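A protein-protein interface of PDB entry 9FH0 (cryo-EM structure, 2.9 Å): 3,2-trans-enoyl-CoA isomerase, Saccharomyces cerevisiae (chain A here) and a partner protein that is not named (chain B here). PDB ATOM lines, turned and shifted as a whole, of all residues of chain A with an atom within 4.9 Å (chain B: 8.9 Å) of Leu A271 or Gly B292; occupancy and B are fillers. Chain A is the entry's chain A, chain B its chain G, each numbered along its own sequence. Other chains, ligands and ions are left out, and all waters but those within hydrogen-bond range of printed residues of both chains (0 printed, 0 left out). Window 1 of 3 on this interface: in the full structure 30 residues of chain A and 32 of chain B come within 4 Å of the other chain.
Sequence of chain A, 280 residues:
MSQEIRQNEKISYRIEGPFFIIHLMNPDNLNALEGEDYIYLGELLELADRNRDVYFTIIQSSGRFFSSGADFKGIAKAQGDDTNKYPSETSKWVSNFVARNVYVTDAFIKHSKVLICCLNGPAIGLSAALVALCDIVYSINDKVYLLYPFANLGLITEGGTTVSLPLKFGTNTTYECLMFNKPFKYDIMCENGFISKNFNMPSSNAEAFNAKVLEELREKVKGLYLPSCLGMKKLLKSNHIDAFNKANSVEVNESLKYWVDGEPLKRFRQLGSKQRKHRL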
ATOM      1  N   LEU A 153      31.012   9.580  21.294  1.00  0.00           N
ATOM      2  CA  LEU A 153      30.702   9.902  19.917  1.00  0.00           C
ATOM      3  C   LEU A 153      31.802   9.510  18.954  1.00  0.00           C
ATOM      4  O   LEU A 153      31.584   9.562  17.750  1.00  0.00           O
ATOM      5  CB  LEU A 153      30.423  11.396  19.769  1.00  0.00           C
ATOM      6  CG  LEU A 153      29.421  12.047  20.713  1.00  0.00           C
ATOM      7  CD1 LEU A 153      29.370  13.519  20.454  1.00  0.00           C
ATOM      8  CD2 LEU A 153      28.063  11.446  20.536  1.00  0.00           C
ATOM      9  N   ARG A 267      27.953   6.090  14.673  1.00  0.00           N
ATOM     10  CA  ARG A 267      27.351   6.111  15.996  1.00  0.00           C
ATOM     11  C   ARG A 267      26.129   7.007  16.026  1.00  0.00           C
ATOM     12  O   ARG A 267      25.154   6.705  16.717  1.00  0.00           O
ATOM     13  CB  ARG A 267      28.375   6.559  17.028  1.00  0.00           C
ATOM     14  CG  ARG A 267      29.427   5.519  17.277  1.00  0.00           C
ATOM     15  CD  ARG A 267      30.425   5.954  18.287  1.00  0.00           C
ATOM     16  NE  ARG A 267      31.199   4.825  18.761  1.00  0.00           N
ATOM     17  CZ  ARG A 267      31.115   4.340  19.986  1.00  0.00           C
ATOM     18  NH1 ARG A 267      30.302   4.891  20.857  1.00  0.00           N
ATOM     19  NH2 ARG A 267      31.844   3.305  20.339  1.00  0.00           N
ATOM     20  N   PHE A 268      26.153   8.108  15.279  1.00  0.00           N
ATOM     21  CA  PHE A 268      24.972   8.957  15.186  1.00  0.00           C
ATOM     22  C   PHE A 268      23.818   8.210  14.549  1.00  0.00           C
ATOM     23  O   PHE A 268      22.682   8.302  15.014  1.00  0.00           O
ATOM     24  CB  PHE A 268      25.285  10.217  14.388  1.00  0.00           C
ATOM     25  CG  PHE A 268      25.999  11.264  15.170  1.00  0.00           C
ATOM     26  CD1 PHE A 268      25.568  11.621  16.422  1.00  0.00           C
ATOM     27  CD2 PHE A 268      27.109  11.883  14.658  1.00  0.00           C
ATOM     28  CE1 PHE A 268      26.228  12.570  17.136  1.00  0.00           C
ATOM     29  CE2 PHE A 268      27.772  12.828  15.375  1.00  0.00           C
ATOM     30  CZ  PHE A 268      27.329  13.172  16.611  1.00  0.00           C
ATOM     31  N   ARG A 269      24.087   7.462  13.483  1.00  0.00           N
ATOM     32  CA  ARG A 269      23.018   6.717  12.836  1.00  0.00           C
ATOM     33  C   ARG A 269      22.424   5.687  13.771  1.00  0.00           C
ATOM     34  O   ARG A 269      21.203   5.570  13.870  1.00  0.00           O
ATOM     35  CB  ARG A 269      23.523   6.043  11.575  1.00  0.00           C
ATOM     36  CG  ARG A 269      23.921   7.020  10.540  1.00  0.00           C
ATOM     37  CD  ARG A 269      23.662   6.504   9.175  1.00  0.00           C
ATOM     38  NE  ARG A 269      24.196   7.415   8.182  1.00  0.00           N
ATOM     39  CZ  ARG A 269      25.421   7.323   7.689  1.00  0.00           C
ATOM     40  NH1 ARG A 269      26.231   6.359   8.104  1.00  0.00           N
ATOM     41  NH2 ARG A 269      25.837   8.196   6.784  1.00  0.00           N
ATOM     42  N   GLN A 270      23.254   4.926  14.464  1.00  0.00           N
ATOM     43  CA  GLN A 270      22.653   3.947  15.356  1.00  0.00           C
ATOM     44  C   GLN A 270      22.187   4.545  16.671  1.00  0.00           C
ATOM     45  O   GLN A 270      21.665   3.814  17.513  1.00  0.00           O
ATOM     46  CB  GLN A 270      23.605   2.779  15.605  1.00  0.00           C
ATOM     47  CG  GLN A 270      24.898   3.113  16.275  1.00  0.00           C
ATOM     48  CD  GLN A 270      25.717   1.870  16.544  1.00  0.00           C
ATOM     49  OE1 GLN A 270      25.211   0.760  16.433  1.00  0.00           O
ATOM     50  NE2 GLN A 270      26.989   2.048  16.890  1.00  0.00           N
ATOM     51  N   LEU A 271      22.353   5.849  16.874  1.00  0.00           N
ATOM     52  CA  LEU A 271      21.700   6.505  17.999  1.00  0.00           C
ATOM     53  C   LEU A 271      20.225   6.699  17.720  1.00  0.00           C
ATOM     54  O   LEU A 271      19.375   6.336  18.533  1.00  0.00           O
ATOM     55  CB  LEU A 271      22.348   7.851  18.280  1.00  0.00           C
ATOM     56  CG  LEU A 271      23.516   7.896  19.238  1.00  0.00           C
ATOM     57  CD1 LEU A 271      23.938   9.314  19.395  1.00  0.00           C
ATOM     58  CD2 LEU A 271      23.110   7.319  20.547  1.00  0.00           C
ATOM     59  N   GLY A 272      19.907   7.292  16.582  1.00  0.00           N
ATOM     60  CA  GLY A 272      18.535   7.519  16.199  1.00  0.00           C
ATOM     61  C   GLY A 272      18.004   6.422  15.314  1.00  0.00           C
ATOM     62  O   GLY A 272      17.531   6.679  14.208  1.00  0.00           O
ATOM     63  N   SER A 273      18.107   5.188  15.782  1.00  0.00           N
ATOM     64  CA  SER A 273      17.636   4.023  15.050  1.00  0.00           C
ATOM     65  C   SER A 273      16.999   3.030  16.011  1.00  0.00           C
ATOM     66  O   SER A 273      17.314   1.841  16.009  1.00  0.00           O
ATOM     67  CB  SER A 273      18.772   3.377  14.275  1.00  0.00           C
ATOM     68  OG  SER A 273      18.310   2.237  13.594  1.00  0.00           O
ATOM     69  N   LYS A 274      16.109   3.517  16.869  1.00  0.00           N
ATOM     70  CA  LYS A 274      15.535   2.722  17.944  1.00  0.00           C
ATOM     71  C   LYS A 274      14.044   2.478  17.761  1.00  0.00           C
ATOM     72  O   LYS A 274      13.286   2.501  18.725  1.00  0.00           O
ATOM     73  CB  LYS A 274      15.776   3.392  19.290  1.00  0.00           C
ATOM     74  CG  LYS A 274      17.220   3.663  19.615  1.00  0.00           C
ATOM     75  CD  LYS A 274      18.060   2.430  19.407  1.00  0.00           C
ATOM     76  CE  LYS A 274      19.452   2.614  19.958  1.00  0.00           C
ATOM     77  NZ  LYS A 274      19.447   2.679  21.440  1.00  0.00           N
ATOM     78  N   ASP B 286      22.115  10.801  29.665  1.00  0.00           N
ATOM     79  CA  ASP B 286      20.935  10.907  28.824  1.00  0.00           C
ATOM     80  C   ASP B 286      21.162  11.861  27.670  1.00  0.00           C
ATOM     81  O   ASP B 286      20.210  12.201  26.971  1.00  0.00           O
ATOM     82  CB  ASP B 286      19.723  11.366  29.624  1.00  0.00           C
ATOM     83  CG  ASP B 286      18.938  10.223  30.200  1.00  0.00           C
ATOM     84  OD1 ASP B 286      19.446   9.087  30.194  1.00  0.00           O
ATOM     85  OD2 ASP B 286      17.797  10.458  30.650  1.00  0.00           O
ATOM     86  N   TYR B 287      22.395  12.312  27.462  1.00  0.00           N
ATOM     87  CA  TYR B 287      22.701  13.109  26.286  1.00  0.00           C
ATOM     88  C   TYR B 287      22.467  12.304  25.022  1.00  0.00           C
ATOM     89  O   TYR B 287      21.696  12.710  24.153  1.00  0.00           O
ATOM     90  CB  TYR B 287      24.134  13.604  26.354  1.00  0.00           C
ATOM     91  CG  TYR B 287      24.532  14.456  25.189  1.00  0.00           C
ATOM     92  CD1 TYR B 287      23.828  15.587  24.874  1.00  0.00           C
ATOM     93  CD2 TYR B 287      25.615  14.130  24.416  1.00  0.00           C
ATOM     94  CE1 TYR B 287      24.183  16.360  23.828  1.00  0.00           C
ATOM     95  CE2 TYR B 287      25.978  14.898  23.370  1.00  0.00           C
ATOM     96  CZ  TYR B 287      25.264  16.016  23.077  1.00  0.00           C
ATOM     97  OH  TYR B 287      25.635  16.801  22.016  1.00  0.00           O
ATOM     98  N   LEU B 288      23.147  11.174  24.888  1.00  0.00           N
ATOM     99  CA  LEU B 288      22.647  10.134  24.011  1.00  0.00           C
ATOM    100  C   LEU B 288      21.286   9.736  24.536  1.00  0.00           C
ATOM    101  O   LEU B 288      21.076   9.700  25.746  1.00  0.00           O
ATOM    102  CB  LEU B 288      23.572   8.931  24.029  1.00  0.00           C
ATOM    103  CG  LEU B 288      25.071   9.178  24.117  1.00  0.00           C
ATOM    104  CD1 LEU B 288      25.765   7.855  24.274  1.00  0.00           C
ATOM    105  CD2 LEU B 288      25.588   9.916  22.907  1.00  0.00           C
ATOM    106  N   LYS B 289      20.362   9.422  23.637  1.00  0.00           N
ATOM    107  CA  LYS B 289      18.931   9.287  23.884  1.00  0.00           C
ATOM    108  C   LYS B 289      18.242  10.640  23.908  1.00  0.00           C
ATOM    109  O   LYS B 289      17.026  10.690  23.826  1.00  0.00           O
ATOM    110  CB  LYS B 289      18.611   8.540  25.195  1.00  0.00           C
ATOM    111  CG  LYS B 289      17.171   8.247  25.484  1.00  0.00           C
ATOM    112  CD  LYS B 289      17.019   7.747  26.897  1.00  0.00           C
ATOM    113  CE  LYS B 289      15.561   7.682  27.278  1.00  0.00           C
ATOM    114  NZ  LYS B 289      14.931   9.009  27.153  1.00  0.00           N
ATOM    115  N   TYR B 290      18.974  11.741  23.942  1.00  0.00           N
ATOM    116  CA  TYR B 290      18.436  13.020  23.518  1.00  0.00           C
ATOM    117  C   TYR B 290      18.869  13.349  22.108  1.00  0.00           C
ATOM    118  O   TYR B 290      18.131  14.007  21.378  1.00  0.00           O
ATOM    119  CB  TYR B 290      18.876  14.133  24.471  1.00  0.00           C
ATOM    120  CG  TYR B 290      18.819  15.516  23.872  1.00  0.00           C
ATOM    121  CD1 TYR B 290      17.623  16.194  23.768  1.00  0.00           C
ATOM    122  CD2 TYR B 290      19.961  16.139  23.407  1.00  0.00           C
ATOM    123  CE1 TYR B 290      17.570  17.442  23.217  1.00  0.00           C
ATOM    124  CE2 TYR B 290      19.912  17.381  22.850  1.00  0.00           C
ATOM    125  CZ  TYR B 290      18.715  18.028  22.761  1.00  0.00           C
ATOM    126  OH  TYR B 290      18.660  19.277  22.208  1.00  0.00           O
ATOM    127  N   LEU B 291      20.046  12.881  21.714  1.00  0.00           N
ATOM    128  CA  LEU B 291      20.473  12.976  20.329  1.00  0.00           C
ATOM    129  C   LEU B 291      19.702  12.025  19.438  1.00  0.00           C
ATOM    130  O   LEU B 291      19.639  12.236  18.229  1.00  0.00           O
ATOM    131  CB  LEU B 291      21.959  12.677  20.214  1.00  0.00           C
ATOM    132  CG  LEU B 291      22.901  13.716  20.774  1.00  0.00           C
ATOM    133  CD1 LEU B 291      24.295  13.267  20.555  1.00  0.00           C
ATOM    134  CD2 LEU B 291      22.648  14.998  20.069  1.00  0.00           C
ATOM    135  N   GLY B 292      19.141  10.963  20.000  1.00  0.00           N
ATOM    136  CA  GLY B 292      18.366  10.051  19.185  1.00  0.00           C
ATOM    137  C   GLY B 292      17.171  10.727  18.551  1.00  0.00           C
ATOM    138  O   GLY B 292      16.846  10.477  17.390  1.00  0.00           O
ATOM    139  N   GLY B 293      16.518  11.603  19.290  1.00  0.00           N
ATOM    140  CA  GLY B 293      15.371  12.305  18.782  1.00  0.00           C
ATOM    141  C   GLY B 293      15.670  13.454  17.857  1.00  0.00           C
ATOM    142  O   GLY B 293      14.751  14.191  17.501  1.00  0.00           O
ATOM    143  N   ARG B 294      16.921  13.634  17.448  1.00  0.00           N
ATOM    144  CA  ARG B 294      17.301  14.803  16.671  1.00  0.00           C
ATOM    145  C   ARG B 294      18.084  14.463  15.420  1.00  0.00           C
ATOM    146  O   ARG B 294      18.000  15.188  14.431  1.00  0.00           O
ATOM    147  CB  ARG B 294      18.133  15.748  17.518  1.00  0.00           C
ATOM    148  CG  ARG B 294      17.475  16.173  18.786  1.00  0.00           C
ATOM    149  CD  ARG B 294      18.014  17.492  19.219  1.00  0.00           C
ATOM    150  NE  ARG B 294      17.264  18.604  18.660  1.00  0.00           N
ATOM    151  CZ  ARG B 294      17.816  19.736  18.249  1.00  0.00           C
ATOM    152  NH1 ARG B 294      19.124  19.894  18.315  1.00  0.00           N
ATOM    153  NH2 ARG B 294      17.061  20.704  17.763  1.00  0.00           N
ATOM    154  N   VAL B 295      18.862  13.383  15.446  1.00  0.00           N
ATOM    155  CA  VAL B 295      19.821  13.169  14.373  1.00  0.00           C
ATOM    156  C   VAL B 295      19.119  12.931  13.049  1.00  0.00           C
ATOM    157  O   VAL B 295      19.632  13.312  11.994  1.00  0.00           O
ATOM    158  CB  VAL B 295      20.781  12.021  14.722  1.00  0.00           C
ATOM    159  CG1 VAL B 295      21.702  12.434  15.831  1.00  0.00           C
ATOM    160  CG2 VAL B 295      20.029  10.799  15.105  1.00  0.00           C
ATOM    161  N   ASN B 296      17.940  12.327  13.066  1.00  0.00           N
ATOM    162  CA  ASN B 296      17.248  12.020  11.824  1.00  0.00           C
ATOM    163  C   ASN B 296      16.603  13.236  11.188  1.00  0.00           C
ATOM    164  O   ASN B 296      16.344  13.220   9.985  1.00  0.00           O
ATOM    165  CB  ASN B 296      16.181  10.967  12.072  1.00  0.00           C
ATOM    166  CG  ASN B 296      16.751   9.598  12.241  1.00  0.00           C
ATOM    167  OD1 ASN B 296      17.585   9.169  11.460  1.00  0.00           O
ATOM    168  ND2 ASN B 296      16.308   8.895  13.266  1.00  0.00           N
ATOM    169  N   GLY B 297      16.325  14.274  11.958  1.00  0.00           N
ATOM    170  CA  GLY B 297      15.723  15.467  11.418  1.00  0.00           C
ATOM    171  C   GLY B 297      14.220  15.334  11.287  1.00  0.00           C
ATOM    172  O   GLY B 297      13.579  14.515  11.940  1.00  0.00           O
ATOM    173  N   GLU B 394       8.357   5.506  17.357  1.00  0.00           N
ATOM    174  CA  GLU B 394       9.626   5.640  16.656  1.00  0.00           C
ATOM    175  C   GLU B 394      10.828   5.608  17.579  1.00  0.00           C
ATOM    176  O   GLU B 394      11.957   5.598  17.091  1.00  0.00           O
ATOM    177  CB  GLU B 394       9.662   6.938  15.866  1.00  0.00           C
ATOM    178  CG  GLU B 394       8.722   6.974  14.713  1.00  0.00           C
ATOM    179  CD  GLU B 394       9.150   6.065  13.603  1.00  0.00           C
ATOM    180  OE1 GLU B 394       8.792   4.875  13.637  1.00  0.00           O
ATOM    181  OE2 GLU B 394       9.846   6.538  12.688  1.00  0.00           O
ATOM    182  N   GLY B 395      10.627   5.605  18.883  1.00  0.00           N
ATOM    183  CA  GLY B 395      11.737   5.579  19.793  1.00  0.00           C
ATOM    184  C   GLY B 395      12.210   6.929  20.268  1.00  0.00           C
ATOM    185  O   GLY B 395      13.218   6.994  20.974  1.00  0.00           O
ATOM    186  N   TYR B 396      11.523   8.007  19.911  1.00  0.00           N
ATOM    187  CA  TYR B 396      11.868   9.336  20.409  1.00  0.00           C
ATOM    188  C   TYR B 396      11.134   9.579  21.723  1.00  0.00           C
ATOM    189  O   TYR B 396      10.177  10.339  21.810  1.00  0.00           O
ATOM    190  CB  TYR B 396      11.519  10.405  19.388  1.00  0.00           C
ATOM    191  CG  TYR B 396      11.964  10.115  17.992  1.00  0.00           C
ATOM    192  CD1 TYR B 396      13.144   9.468  17.748  1.00  0.00           C
ATOM    193  CD2 TYR B 396      11.208  10.502  16.921  1.00  0.00           C
ATOM    194  CE1 TYR B 396      13.551   9.206  16.475  1.00  0.00           C
ATOM    195  CE2 TYR B 396      11.606  10.246  15.652  1.00  0.00           C
ATOM    196  CZ  TYR B 396      12.779   9.598  15.433  1.00  0.00           C
ATOM    197  OH  TYR B 396      13.184   9.340  14.155  1.00  0.00           O
ATOM    198  N   ASP B 397      11.616   8.916  22.769  1.00  0.00           N
ATOM    199  CA  ASP B 397      10.894   8.948  24.031  1.00  0.00           C
ATOM    200  C   ASP B 397      10.897  10.330  24.664  1.00  0.00           C
ATOM    201  O   ASP B 397       9.911  10.713  25.298  1.00  0.00           O
ATOM    202  CB  ASP B 397      11.487   7.928  24.991  1.00  0.00           C
ATOM    203  CG  ASP B 397      11.493   6.538  24.418  1.00  0.00           C
ATOM    204  OD1 ASP B 397      11.023   6.376  23.280  1.00  0.00           O
ATOM    205  OD2 ASP B 397      11.969   5.610  25.099  1.00  0.00           O
ATOM    206  N   MET B 398      11.972  11.097  24.506  1.00  0.00           N
ATOM    207  CA  MET B 398      12.043  12.394  25.172  1.00  0.00           C
ATOM    208  C   MET B 398      11.151  13.427  24.499  1.00  0.00           C
ATOM    209  O   MET B 398      10.534  14.254  25.180  1.00  0.00           O
ATOM    210  CB  MET B 398      13.486  12.882  25.220  1.00  0.00           C
ATOM    211  CG  MET B 398      14.354  12.111  26.182  1.00  0.00           C
ATOM    212  SD  MET B 398      15.686  13.100  26.839  1.00  0.00           S
ATOM    213  CE  MET B 398      16.100  12.149  28.284  1.00  0.00           C
ATOM    214  N   SER B 399      11.072  13.403  23.167  1.00  0.00           N
ATOM    215  CA  SER B 399      10.103  14.242  22.477  1.00  0.00           C
ATOM    216  C   SER B 399       8.688  13.892  22.903  1.00  0.00           C
ATOM    217  O   SER B 399       7.838  14.774  23.056  1.00  0.00           O
ATOM    218  CB  SER B 399      10.255  14.089  20.970  1.00  0.00           C
ATOM    219  OG  SER B 399      11.596  14.244  20.576  1.00  0.00           O
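The backbone carbonyl oxygen (O) of Gly A272 sits at hydrogen-bond distance from the side-chain amide nitrogen (ND2) of Asn B296 (2.7 Å).
The side-chain amide nitrogen of Asn B296 sits at hydrogen-bond distance from the side-chain hydroxyl of Tyr B396.
Among the printed residues, merely in contact across the chains: Leu A153 with Leu B288, Phe A268 with Leu B291, Phe A268 with Val B295, Leu A271 with Leu B288, Leu A271 with Leu B291, Leu A271 with Gly B292, Gly A272 with Gly B292, Gly A272 with Val B295, Lys A274 with Glu B394 and Lys A274 with Gly B395.
Of the printed residues of chain B, Leu A271 touches Leu B288 (3.9 Å), Leu B291 (3.99 Å) and Gly B292 (3.9 Å).
Tyr B287 touches none of the printed residues of chain A.
Gly B292 touches two residues of chain A.
Arg B294 touches none of the printed residues of chain A.
Of the printed residues of chain A, Val B295 touches Phe A268 and Gly A272.
Of the printed residues of chain A, Asn B296 touches Gly A272.
Of the printed residues of chain A, Glu B394 touches Lys A274.
The nearest printed residue of chain B that does not touch Leu A271 is Lys B289 (4.6 Å).
Hydrophobic or aromatic side chains of chain A that line the printed part of chain B: Leu A153, Phe A268 and Leu A271.
Hydrophobic or aromatic side chains of chain B that line the printed part of chain A: Leu B288, Leu B291 and Val B295.
Among the printed residues, no Asp or Glu carboxylate lies within 4 Å of a Lys or Arg side-chain nitrogen of the other chain.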
